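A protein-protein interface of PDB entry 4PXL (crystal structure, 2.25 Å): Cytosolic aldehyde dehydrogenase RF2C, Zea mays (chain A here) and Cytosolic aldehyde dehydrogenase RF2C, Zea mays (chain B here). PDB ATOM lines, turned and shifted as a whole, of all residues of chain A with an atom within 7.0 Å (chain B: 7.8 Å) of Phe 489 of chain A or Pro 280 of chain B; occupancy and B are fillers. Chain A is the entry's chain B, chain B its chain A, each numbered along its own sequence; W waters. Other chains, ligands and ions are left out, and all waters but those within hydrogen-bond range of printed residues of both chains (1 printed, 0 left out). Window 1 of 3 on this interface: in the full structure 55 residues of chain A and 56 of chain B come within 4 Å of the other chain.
O of Ser 487 of chain A lies within hydrogen-bond range of N of Leu 285 of chain A. The backbone NH of Leu 283 of chain A lies within hydrogen-bond range of the backbone carbonyl oxygen of Phe 489 of chain A (2.9 Å). The side-chain amino group (NZ) of Lys 279 of chain B sits at hydrogen-bond distance from the backbone carbonyl oxygen (O) of Ala 249 of chain B. N of Leu 278 of chain B lies within hydrogen-bond range of O of Ala 273 of chain B (2.8 Å). O of Val 254 of chain B lies within hydrogen-bond range of ND2 of Asn 277 of chain B (2.8 Å). N of Val 257 of chain B sits at hydrogen-bond distance from O of Pro 280 of chain B.
Among the printed residues, pairs that only touch across the chains: Met 486 of chain A with Asn 277 of chain B, Phe 489 of chain A with Leu 278 of chain B, Tyr 484 of chain A with Gln 503 of chain B, Met 270 of chain A with Lys 279 of chain B, Met 270 of chain A with Ala 274 of chain B, Leu 285 of chain A with Leu 278 of chain B, Leu 283 of chain A with Leu 278 of chain B, Phe 489 of chain A with Pro 280 of chain B, Met 270 of chain A with Ala 273 of chain B, Pro 280 of chain A with Phe 489 of chain B and Met 270 of chain A with Met 270 of chain B.
Of the printed residues of chain B, Met 270 of chain A touches Met 270, Ala 273, Ala 274 and Lys 279. Of the printed residues of chain B, Pro 280 of chain A touches Phe 489 (3.9 Å). Printed residues of chain B within 4 Å of Leu 283 of chain A: Leu 278 (3.8 Å). Gly 482 of chain A touches none of the printed residues of chain B. Printed residues of chain B within 4 Å of Met 486 of chain A: Asn 277 (3.2 Å). No residue of chain B comes within 4 Å of Gly 488 of chain A. Phe 489 of chain A touches two residues of chain B. No residue of chain B comes within 4 Å of Gly 490 of chain A. Ser 258 of chain B touches none of the printed residues of chain A. Printed residues of chain A within 4 Å of Asn 277 of chain B: Met 486 (3.2 Å). Of chain A, only Phe 489 (3.8 Å) comes within 4 Å of Pro 280 of chain B. The nearest residue of chain B that does not touch Phe 489 of chain A is Lys 279 of chain B (4.1 Å). The nearest printed residue of chain A that does not touch Phe 489 of chain B is Val 281 of chain A (5.5 Å).
Of the 21 printed residues of chain B, 9 touch a printed residue of chain A. Hydrophobic or aromatic side chains of chain B within 4 Å of the printed part of chain A: Met 270, Ala 273, Ala 274, Leu 278, Pro 280 and Phe 489. Along chain B the printed residues that touch a printed residue of chain A span positions 270 to 503.
Water W1 bridges OE1 of Gln 503 of chain B (3.3 Å) and NZ of Lys 491 of chain A (3.3 Å).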
ATOM      1  N   PHE A 259      17.719 -15.013  16.632  1.00  0.00           N
ATOM      2  CA  PHE A 259      16.525 -14.698  15.853  1.00  0.00           C
ATOM      3  C   PHE A 259      15.246 -14.628  16.735  1.00  0.00           C
ATOM      4  O   PHE A 259      14.995 -15.511  17.568  1.00  0.00           O
ATOM      5  CB  PHE A 259      16.344 -15.710  14.697  1.00  0.00           C
ATOM      6  CG  PHE A 259      14.977 -15.659  14.036  1.00  0.00           C
ATOM      7  CD1 PHE A 259      14.742 -14.829  12.945  1.00  0.00           C
ATOM      8  CD2 PHE A 259      13.912 -16.408  14.536  1.00  0.00           C
ATOM      9  CE1 PHE A 259      13.465 -14.723  12.388  1.00  0.00           C
ATOM     10  CE2 PHE A 259      12.640 -16.318  13.961  1.00  0.00           C
ATOM     11  CZ  PHE A 259      12.425 -15.476  12.894  1.00  0.00           C
ATOM     12  N   MET A 270      17.221 -22.023  11.721  1.00  0.00           N
ATOM     13  CA  MET A 270      17.888 -23.186  12.324  1.00  0.00           C
ATOM     14  C   MET A 270      18.425 -24.118  11.237  1.00  0.00           C
ATOM     15  O   MET A 270      19.565 -24.552  11.314  1.00  0.00           O
ATOM     16  CB  MET A 270      16.943 -23.915  13.316  1.00  0.00           C
ATOM     17  CG  MET A 270      17.674 -24.830  14.291  1.00  0.00           C
ATOM     18  SD  MET A 270      16.569 -25.627  15.497  1.00  0.00           S
ATOM     19  CE  MET A 270      17.729 -26.672  16.357  1.00  0.00           C
ATOM     20  N   PRO A 280      25.834 -21.898  16.218  1.00  0.00           N
ATOM     21  CA  PRO A 280      24.733 -22.025  17.164  1.00  0.00           C
ATOM     22  C   PRO A 280      23.741 -20.907  16.903  1.00  0.00           C
ATOM     23  O   PRO A 280      24.066 -19.839  16.378  1.00  0.00           O
ATOM     24  CB  PRO A 280      25.388 -21.873  18.521  1.00  0.00           C
ATOM     25  CG  PRO A 280      26.718 -21.173  18.255  1.00  0.00           C
ATOM     26  CD  PRO A 280      27.098 -21.491  16.880  1.00  0.00           C
ATOM     27  N   VAL A 281      22.529 -21.161  17.314  1.00  0.00           N
ATOM     28  CA  VAL A 281      21.361 -20.346  17.088  1.00  0.00           C
ATOM     29  C   VAL A 281      20.575 -20.240  18.398  1.00  0.00           C
ATOM     30  O   VAL A 281      20.522 -21.202  19.162  1.00  0.00           O
ATOM     31  CB  VAL A 281      20.591 -21.133  15.985  1.00  0.00           C
ATOM     32  CG1 VAL A 281      19.113 -20.921  16.043  1.00  0.00           C
ATOM     33  CG2 VAL A 281      21.133 -20.829  14.591  1.00  0.00           C
ATOM     34  N   SER A 282      19.975 -19.075  18.655  1.00  0.00           N
ATOM     35  CA  SER A 282      19.053 -18.844  19.769  1.00  0.00           C
ATOM     36  C   SER A 282      17.788 -18.272  19.117  1.00  0.00           C
ATOM     37  O   SER A 282      17.892 -17.406  18.238  1.00  0.00           O
ATOM     38  CB  SER A 282      19.651 -17.907  20.822  1.00  0.00           C
ATOM     39  OG  SER A 282      19.648 -16.558  20.391  1.00  0.00           O
ATOM     40  N   LEU A 283      16.604 -18.793  19.502  1.00  0.00           N
ATOM     41  CA  LEU A 283      15.304 -18.442  18.894  1.00  0.00           C
ATOM     42  C   LEU A 283      14.224 -18.087  19.900  1.00  0.00           C
ATOM     43  O   LEU A 283      13.997 -18.845  20.829  1.00  0.00           O
ATOM     44  CB  LEU A 283      14.736 -19.620  18.042  1.00  0.00           C
ATOM     45  CG  LEU A 283      15.619 -20.398  17.048  1.00  0.00           C
ATOM     46  CD1 LEU A 283      14.881 -21.665  16.547  1.00  0.00           C
ATOM     47  CD2 LEU A 283      16.001 -19.538  15.854  1.00  0.00           C
ATOM     48  N   GLU A 284      13.515 -16.974  19.671  1.00  0.00           N
ATOM     49  CA  GLU A 284      12.346 -16.572  20.444  1.00  0.00           C
ATOM     50  C   GLU A 284      11.240 -16.576  19.404  1.00  0.00           C
ATOM     51  O   GLU A 284      11.249 -15.764  18.463  1.00  0.00           O
ATOM     52  CB  GLU A 284      12.555 -15.199  21.110  1.00  0.00           C
ATOM     53  CG  GLU A 284      11.513 -14.866  22.185  1.00  0.00           C
ATOM     54  CD  GLU A 284      10.307 -14.093  21.675  1.00  0.00           C
ATOM     55  OE1 GLU A 284      10.317 -12.842  21.769  1.00  0.00           O
ATOM     56  OE2 GLU A 284       9.362 -14.736  21.161  1.00  0.00           O
ATOM     57  N   LEU A 285      10.344 -17.565  19.497  1.00  0.00           N
ATOM     58  CA  LEU A 285       9.327 -17.784  18.452  1.00  0.00           C
ATOM     59  C   LEU A 285       7.858 -17.486  18.766  1.00  0.00           C
ATOM     60  O   LEU A 285       6.966 -17.953  18.057  1.00  0.00           O
ATOM     61  CB  LEU A 285       9.473 -19.184  17.857  1.00  0.00           C
ATOM     62  CG  LEU A 285      10.870 -19.599  17.480  1.00  0.00           C
ATOM     63  CD1 LEU A 285      10.961 -21.114  17.303  1.00  0.00           C
ATOM     64  CD2 LEU A 285      11.388 -18.781  16.283  1.00  0.00           C
ATOM     65  N   GLY A 482      13.055 -16.281  27.912  1.00  0.00           N
ATOM     66  CA  GLY A 482      13.146 -17.246  26.830  1.00  0.00           C
ATOM     67  C   GLY A 482      12.126 -18.341  26.993  1.00  0.00           C
ATOM     68  O   GLY A 482      11.680 -18.611  28.106  1.00  0.00           O
ATOM     69  N   GLY A 483      11.774 -18.973  25.883  1.00  0.00           N
ATOM     70  CA  GLY A 483      10.729 -19.978  25.857  1.00  0.00           C
ATOM     71  C   GLY A 483      11.124 -21.412  26.076  1.00  0.00           C
ATOM     72  O   GLY A 483      12.304 -21.764  26.138  1.00  0.00           O
ATOM     73  N   TYR A 484      10.091 -22.229  26.251  1.00  0.00           N
ATOM     74  CA  TYR A 484      10.120 -23.679  26.351  1.00  0.00           C
ATOM     75  C   TYR A 484       9.415 -24.120  25.053  1.00  0.00           C
ATOM     76  O   TYR A 484       8.764 -23.294  24.369  1.00  0.00           O
ATOM     77  CB  TYR A 484       9.220 -24.132  27.519  1.00  0.00           C
ATOM     78  CG  TYR A 484       9.791 -24.102  28.926  1.00  0.00           C
ATOM     79  CD1 TYR A 484      10.649 -23.083  29.336  1.00  0.00           C
ATOM     80  CD2 TYR A 484       9.377 -25.023  29.881  1.00  0.00           C
ATOM     81  CE1 TYR A 484      11.124 -23.021  30.646  1.00  0.00           C
ATOM     82  CE2 TYR A 484       9.841 -24.969  31.194  1.00  0.00           C
ATOM     83  CZ  TYR A 484      10.699 -23.957  31.577  1.00  0.00           C
ATOM     84  OH  TYR A 484      11.156 -23.939  32.869  1.00  0.00           O
ATOM     85  N   LYS A 485       9.501 -25.426  24.734  1.00  0.00           N
ATOM     86  CA  LYS A 485       8.750 -26.042  23.642  1.00  0.00           C
ATOM     87  C   LYS A 485       8.893 -25.298  22.327  1.00  0.00           C
ATOM     88  O   LYS A 485      10.003 -24.930  21.991  1.00  0.00           O
ATOM     89  CB  LYS A 485       7.277 -26.196  24.081  1.00  0.00           C
ATOM     90  CG  LYS A 485       7.093 -27.136  25.287  1.00  0.00           C
ATOM     91  CD  LYS A 485       5.822 -26.874  26.117  1.00  0.00           C
ATOM     92  CE  LYS A 485       4.523 -27.214  25.406  1.00  0.00           C
ATOM     93  NZ  LYS A 485       3.330 -27.077  26.334  1.00  0.00           N
ATOM     94  N   MET A 486       7.808 -25.047  21.585  1.00  0.00           N
ATOM     95  CA  MET A 486       7.933 -24.332  20.305  1.00  0.00           C
ATOM     96  C   MET A 486       8.107 -22.804  20.388  1.00  0.00           C
ATOM     97  O   MET A 486       8.204 -22.132  19.356  1.00  0.00           O
ATOM     98  CB  MET A 486       6.920 -24.790  19.266  1.00  0.00           C
ATOM     99  CG  MET A 486       7.115 -26.221  18.882  1.00  0.00           C
ATOM    100  SD  MET A 486       6.079 -26.640  17.464  1.00  0.00           S
ATOM    101  CE  MET A 486       5.916 -28.336  17.739  1.00  0.00           C
ATOM    102  N   SER A 487       8.270 -22.268  21.615  1.00  0.00           N
ATOM    103  CA  SER A 487       8.583 -20.846  21.779  1.00  0.00           C
ATOM    104  C   SER A 487      10.073 -20.575  21.530  1.00  0.00           C
ATOM    105  O   SER A 487      10.496 -19.425  21.387  1.00  0.00           O
ATOM    106  CB  SER A 487       8.078 -20.334  23.116  1.00  0.00           C
ATOM    107  OG  SER A 487       6.656 -20.362  23.072  1.00  0.00           O
ATOM    108  N   GLY A 488      10.840 -21.653  21.380  1.00  0.00           N
ATOM    109  CA  GLY A 488      12.253 -21.582  21.065  1.00  0.00           C
ATOM    110  C   GLY A 488      13.137 -21.906  22.247  1.00  0.00           C
ATOM    111  O   GLY A 488      12.727 -22.614  23.176  1.00  0.00           O
ATOM    112  N   PHE A 489      14.383 -21.423  22.185  1.00  0.00           N
ATOM    113  CA  PHE A 489      15.401 -21.683  23.202  1.00  0.00           C
ATOM    114  C   PHE A 489      16.448 -20.570  23.215  1.00  0.00           C
ATOM    115  O   PHE A 489      16.620 -19.881  22.218  1.00  0.00           O
ATOM    116  CB  PHE A 489      16.058 -23.058  22.971  1.00  0.00           C
ATOM    117  CG  PHE A 489      16.432 -23.322  21.538  1.00  0.00           C
ATOM    118  CD1 PHE A 489      17.652 -22.879  21.030  1.00  0.00           C
ATOM    119  CD2 PHE A 489      15.588 -24.056  20.703  1.00  0.00           C
ATOM    120  CE1 PHE A 489      17.997 -23.109  19.686  1.00  0.00           C
ATOM    121  CE2 PHE A 489      15.935 -24.295  19.367  1.00  0.00           C
ATOM    122  CZ  PHE A 489      17.141 -23.816  18.866  1.00  0.00           C
ATOM    123  N   GLY A 490      17.136 -20.439  24.344  1.00  0.00           N
ATOM    124  CA  GLY A 490      18.127 -19.399  24.588  1.00  0.00           C
ATOM    125  C   GLY A 490      17.440 -18.259  25.302  1.00  0.00           C
ATOM    126  O   GLY A 490      16.214 -18.124  25.220  1.00  0.00           O
ATOM    127  N   LYS A 491      18.210 -17.430  26.004  1.00  0.00           N
ATOM    128  CA  LYS A 491      17.660 -16.306  26.756  1.00  0.00           C
ATOM    129  C   LYS A 491      18.073 -14.935  26.258  1.00  0.00           C
ATOM    130  O   LYS A 491      19.200 -14.731  25.819  1.00  0.00           O
ATOM    131  CB  LYS A 491      18.024 -16.425  28.250  1.00  0.00           C
ATOM    132  CG  LYS A 491      17.627 -17.743  28.941  1.00  0.00           C
ATOM    133  CD  LYS A 491      16.125 -17.847  29.166  1.00  0.00           C
ATOM    134  CE  LYS A 491      15.823 -19.103  29.922  1.00  0.00           C
ATOM    135  NZ  LYS A 491      14.369 -19.342  29.994  1.00  0.00           N
ATOM    136  N   LYS A 500      25.438 -16.012  26.247  1.00  0.00           N
ATOM    137  CA  LYS A 500      25.343 -16.609  24.911  1.00  0.00           C
ATOM    138  C   LYS A 500      26.277 -15.991  23.865  1.00  0.00           C
ATOM    139  O   LYS A 500      26.502 -16.591  22.825  1.00  0.00           O
ATOM    140  CB  LYS A 500      23.891 -16.818  24.449  1.00  0.00           C
ATOM    141  CG  LYS A 500      23.198 -15.652  23.807  1.00  0.00           C
ATOM    142  CD  LYS A 500      21.724 -15.994  23.646  1.00  0.00           C
ATOM    143  CE  LYS A 500      20.938 -14.858  23.047  1.00  0.00           C
ATOM    144  NZ  LYS A 500      19.478 -15.165  22.988  1.00  0.00           N
ATOM    145  N   VAL B 175      14.595 -30.612  31.861  1.00  0.00           N
ATOM    146  CA  VAL B 175      14.085 -30.334  30.498  1.00  0.00           C
ATOM    147  C   VAL B 175      12.898 -31.242  30.126  1.00  0.00           C
ATOM    148  O   VAL B 175      11.919 -30.777  29.529  1.00  0.00           O
ATOM    149  CB  VAL B 175      15.221 -30.357  29.436  1.00  0.00           C
ATOM    150  CG1 VAL B 175      14.688 -30.605  28.049  1.00  0.00           C
ATOM    151  CG2 VAL B 175      16.010 -29.055  29.447  1.00  0.00           C
ATOM    152  N   GLY B 179      16.846 -37.079  24.152  1.00  0.00           N
ATOM    153  CA  GLY B 179      17.348 -38.072  23.226  1.00  0.00           C
ATOM    154  C   GLY B 179      18.846 -37.955  23.087  1.00  0.00           C
ATOM    155  O   GLY B 179      19.362 -36.852  22.905  1.00  0.00           O
ATOM    156  N   ALA B 249      16.025 -37.795  16.651  1.00  0.00           N
ATOM    157  CA  ALA B 249      16.263 -36.405  16.228  1.00  0.00           C
ATOM    158  C   ALA B 249      14.970 -35.704  15.766  1.00  0.00           C
ATOM    159  O   ALA B 249      14.772 -34.551  16.098  1.00  0.00           O
ATOM    160  CB  ALA B 249      17.301 -36.385  15.100  1.00  0.00           C
ATOM    161  N   VAL B 254      10.259 -35.325  22.079  1.00  0.00           N
ATOM    162  CA  VAL B 254      11.596 -35.289  22.677  1.00  0.00           C
ATOM    163  C   VAL B 254      11.901 -33.799  22.845  1.00  0.00           C
ATOM    164  O   VAL B 254      11.744 -33.013  21.906  1.00  0.00           O
ATOM    165  CB  VAL B 254      12.646 -36.027  21.795  1.00  0.00           C
ATOM    166  CG1 VAL B 254      14.081 -35.713  22.246  1.00  0.00           C
ATOM    167  CG2 VAL B 254      12.399 -37.531  21.815  1.00  0.00           C
ATOM    168  N   ASP B 255      12.264 -33.416  24.055  1.00  0.00           N
ATOM    169  CA  ASP B 255      12.484 -32.015  24.418  1.00  0.00           C
ATOM    170  C   ASP B 255      13.838 -31.469  24.023  1.00  0.00           C
ATOM    171  O   ASP B 255      13.965 -30.264  23.777  1.00  0.00           O
ATOM    172  CB  ASP B 255      12.175 -31.793  25.900  1.00  0.00           C
ATOM    173  CG  ASP B 255      10.752 -32.239  26.288  1.00  0.00           C
ATOM    174  OD1 ASP B 255       9.778 -31.665  25.749  1.00  0.00           O
ATOM    175  OD2 ASP B 255      10.621 -33.183  27.102  1.00  0.00           O
ATOM    176  N   LYS B 256      14.847 -32.340  23.960  1.00  0.00           N
ATOM    177  CA  LYS B 256      16.216 -31.910  23.677  1.00  0.00           C
ATOM    178  C   LYS B 256      16.966 -33.085  23.143  1.00  0.00           C
ATOM    179  O   LYS B 256      16.678 -34.223  23.528  1.00  0.00           O
ATOM    180  CB  LYS B 256      16.899 -31.417  24.994  1.00  0.00           C
ATOM    181  CG  LYS B 256      18.051 -30.455  24.778  1.00  0.00           C
ATOM    182  CD  LYS B 256      19.179 -30.631  25.763  1.00  0.00           C
ATOM    183  CE  LYS B 256      20.454 -29.940  25.287  1.00  0.00           C
ATOM    184  NZ  LYS B 256      21.344 -30.861  24.515  1.00  0.00           N
ATOM    185  N   VAL B 257      17.920 -32.825  22.253  1.00  0.00           N
ATOM    186  CA  VAL B 257      18.762 -33.870  21.685  1.00  0.00           C
ATOM    187  C   VAL B 257      20.233 -33.503  21.796  1.00  0.00           C
ATOM    188  O   VAL B 257      20.614 -32.331  21.632  1.00  0.00           O
ATOM    189  CB  VAL B 257      18.338 -34.330  20.246  1.00  0.00           C
ATOM    190  CG1 VAL B 257      18.522 -33.233  19.220  1.00  0.00           C
ATOM    191  CG2 VAL B 257      19.063 -35.601  19.789  1.00  0.00           C
ATOM    192  N   SER B 258      21.047 -34.508  22.111  1.00  0.00           N
ATOM    193  CA  SER B 258      22.501 -34.376  22.149  1.00  0.00           C
ATOM    194  C   SER B 258      23.038 -35.405  21.197  1.00  0.00           C
ATOM    195  O   SER B 258      22.589 -36.572  21.217  1.00  0.00           O
ATOM    196  CB  SER B 258      23.037 -34.622  23.547  1.00  0.00           C
ATOM    197  OG  SER B 258      24.309 -34.016  23.670  1.00  0.00           O
ATOM    198  N   VAL B 269      20.849 -33.914  12.108  1.00  0.00           N
ATOM    199  CA  VAL B 269      20.260 -33.804  13.446  1.00  0.00           C
ATOM    200  C   VAL B 269      19.724 -32.393  13.693  1.00  0.00           C
ATOM    201  O   VAL B 269      18.581 -32.252  14.118  1.00  0.00           O
ATOM    202  CB  VAL B 269      21.226 -34.297  14.552  1.00  0.00           C
ATOM    203  CG1 VAL B 269      20.689 -33.971  15.961  1.00  0.00           C
ATOM    204  CG2 VAL B 269      21.483 -35.795  14.391  1.00  0.00           C
ATOM    205  N   MET B 270      20.522 -31.367  13.401  1.00  0.00           N
ATOM    206  CA  MET B 270      20.121 -29.970  13.596  1.00  0.00           C
ATOM    207  C   MET B 270      18.920 -29.630  12.717  1.00  0.00           C
ATOM    208  O   MET B 270      17.955 -29.030  13.199  1.00  0.00           O
ATOM    209  CB  MET B 270      21.297 -29.002  13.363  1.00  0.00           C
ATOM    210  CG  MET B 270      21.050 -27.586  13.923  1.00  0.00           C
ATOM    211  SD  MET B 270      22.507 -26.506  13.737  1.00  0.00           S
ATOM    212  CE  MET B 270      21.878 -24.985  14.505  1.00  0.00           C
ATOM    213  N   ALA B 273      15.615 -31.351  14.070  1.00  0.00           N
ATOM    214  CA  ALA B 273      15.082 -30.606  15.197  1.00  0.00           C
ATOM    215  C   ALA B 273      14.264 -29.405  14.672  1.00  0.00           C
ATOM    216  O   ALA B 273      13.116 -29.206  15.090  1.00  0.00           O
ATOM    217  CB  ALA B 273      16.238 -30.117  16.038  1.00  0.00           C
ATOM    218  N   ALA B 274      14.850 -28.629  13.737  1.00  0.00           N
ATOM    219  CA  ALA B 274      14.217 -27.471  13.108  1.00  0.00           C
ATOM    220  C   ALA B 274      12.887 -27.845  12.397  1.00  0.00           C
ATOM    221  O   ALA B 274      11.924 -27.081  12.458  1.00  0.00           O
ATOM    222  CB  ALA B 274      15.179 -26.840  12.110  1.00  0.00           C
ATOM    223  N   ASN B 277       9.991 -30.255  16.146  1.00  0.00           N
ATOM    224  CA  ASN B 277       9.416 -29.440  17.218  1.00  0.00           C
ATOM    225  C   ASN B 277      10.309 -28.283  17.694  1.00  0.00           C
ATOM    226  O   ASN B 277      10.013 -27.674  18.713  1.00  0.00           O
ATOM    227  CB  ASN B 277       9.042 -30.352  18.395  1.00  0.00           C
ATOM    228  CG  ASN B 277      10.210 -31.085  19.014  1.00  0.00           C
ATOM    229  OD1 ASN B 277      11.308 -31.161  18.462  1.00  0.00           O
ATOM    230  ND2 ASN B 277       9.997 -31.660  20.180  1.00  0.00           N
ATOM    231  N   LEU B 278      11.404 -27.981  16.986  1.00  0.00           N
ATOM    232  CA  LEU B 278      12.315 -26.891  17.385  1.00  0.00           C
ATOM    233  C   LEU B 278      12.989 -27.155  18.745  1.00  0.00           C
ATOM    234  O   LEU B 278      13.260 -26.236  19.535  1.00  0.00           O
ATOM    235  CB  LEU B 278      11.636 -25.506  17.292  1.00  0.00           C
ATOM    236  CG  LEU B 278      11.341 -25.077  15.874  1.00  0.00           C
ATOM    237  CD1 LEU B 278       9.994 -24.384  15.761  1.00  0.00           C
ATOM    238  CD2 LEU B 278      12.521 -24.291  15.263  1.00  0.00           C
ATOM    239  N   LYS B 279      13.267 -28.443  19.010  1.00  0.00           N
ATOM    240  CA  LYS B 279      13.977 -28.851  20.212  1.00  0.00           C
ATOM    241  C   LYS B 279      15.414 -28.309  20.106  1.00  0.00           C
ATOM    242  O   LYS B 279      16.012 -28.381  19.021  1.00  0.00           O
ATOM    243  CB  LYS B 279      14.017 -30.394  20.330  1.00  0.00           C
ATOM    244  CG  LYS B 279      14.598 -31.115  19.091  1.00  0.00           C
ATOM    245  CD  LYS B 279      14.897 -32.597  19.246  1.00  0.00           C
ATOM    246  CE  LYS B 279      13.686 -33.512  19.185  1.00  0.00           C
ATOM    247  NZ  LYS B 279      12.918 -33.395  17.921  1.00  0.00           N
ATOM    248  N   PRO B 280      16.018 -27.795  21.203  1.00  0.00           N
ATOM    249  CA  PRO B 280      17.439 -27.403  21.104  1.00  0.00           C
ATOM    250  C   PRO B 280      18.285 -28.664  20.931  1.00  0.00           C
ATOM    251  O   PRO B 280      17.882 -29.766  21.351  1.00  0.00           O
ATOM    252  CB  PRO B 280      17.738 -26.724  22.460  1.00  0.00           C
ATOM    253  CG  PRO B 280      16.664 -27.175  23.377  1.00  0.00           C
ATOM    254  CD  PRO B 280      15.479 -27.622  22.565  1.00  0.00           C
ATOM    255  N   VAL B 281      19.440 -28.507  20.283  1.00  0.00           N
ATOM    256  CA  VAL B 281      20.414 -29.576  20.069  1.00  0.00           C
ATOM    257  C   VAL B 281      21.765 -29.168  20.664  1.00  0.00           C
ATOM    258  O   VAL B 281      22.056 -27.987  20.853  1.00  0.00           O
ATOM    259  CB  VAL B 281      20.603 -29.986  18.569  1.00  0.00           C
ATOM    260  CG1 VAL B 281      19.297 -30.301  17.881  1.00  0.00           C
ATOM    261  CG2 VAL B 281      21.387 -28.945  17.773  1.00  0.00           C
ATOM    262  N   SER B 282      22.622 -30.143  20.857  1.00  0.00           N
ATOM    263  CA  SER B 282      24.009 -29.901  21.154  1.00  0.00           C
ATOM    264  C   SER B 282      24.770 -30.907  20.310  1.00  0.00           C
ATOM    265  O   SER B 282      24.287 -32.020  20.056  1.00  0.00           O
ATOM    266  CB  SER B 282      24.332 -29.895  22.654  1.00  0.00           C
ATOM    267  OG  SER B 282      24.061 -31.103  23.328  1.00  0.00           O
ATOM    268  N   PHE B 489      28.744 -27.178  19.098  1.00  0.00           N
ATOM    269  CA  PHE B 489      28.415 -26.289  20.221  1.00  0.00           C
ATOM    270  C   PHE B 489      27.764 -27.094  21.351  1.00  0.00           C
ATOM    271  O   PHE B 489      27.198 -28.154  21.118  1.00  0.00           O
ATOM    272  CB  PHE B 489      27.493 -25.150  19.759  1.00  0.00           C
ATOM    273  CG  PHE B 489      26.357 -25.615  18.869  1.00  0.00           C
ATOM    274  CD1 PHE B 489      25.170 -26.094  19.416  1.00  0.00           C
ATOM    275  CD2 PHE B 489      26.450 -25.508  17.486  1.00  0.00           C
ATOM    276  CE1 PHE B 489      24.112 -26.497  18.587  1.00  0.00           C
ATOM    277  CE2 PHE B 489      25.392 -25.904  16.664  1.00  0.00           C
ATOM    278  CZ  PHE B 489      24.231 -26.395  17.222  1.00  0.00           C
ATOM    279  N   LYS B 500      22.750 -27.976  30.680  1.00  0.00           N
ATOM    280  CA  LYS B 500      21.989 -28.150  29.444  1.00  0.00           C
ATOM    281  C   LYS B 500      20.759 -29.064  29.578  1.00  0.00           C
ATOM    282  O   LYS B 500      19.924 -29.065  28.697  1.00  0.00           O
ATOM    283  CB  LYS B 500      22.890 -28.431  28.228  1.00  0.00           C
ATOM    284  CG  LYS B 500      23.284 -29.864  27.969  1.00  0.00           C
ATOM    285  CD  LYS B 500      24.373 -29.887  26.873  1.00  0.00           C
ATOM    286  CE  LYS B 500      24.859 -31.290  26.593  1.00  0.00           C
ATOM    287  NZ  LYS B 500      25.956 -31.333  25.596  1.00  0.00           N
ATOM    288  N   GLN B 503      16.042 -26.390  32.503  1.00  0.00           N
ATOM    289  CA  GLN B 503      15.450 -25.182  31.943  1.00  0.00           C
ATOM    290  C   GLN B 503      15.599 -24.128  33.037  1.00  0.00           C
ATOM    291  O   GLN B 503      15.611 -24.475  34.209  1.00  0.00           O
ATOM    292  CB  GLN B 503      13.942 -25.377  31.733  1.00  0.00           C
ATOM    293  CG  GLN B 503      13.516 -26.516  30.807  1.00  0.00           C
ATOM    294  CD  GLN B 503      13.301 -26.061  29.389  1.00  0.00           C
ATOM    295  OE1 GLN B 503      13.944 -25.110  28.887  1.00  0.00           O
ATOM    296  NE2 GLN B 503      12.389 -26.753  28.710  1.00  0.00           N
HETATM  297  O   HOH W   1      15.607 -22.445  29.922  1.00  0.00           O
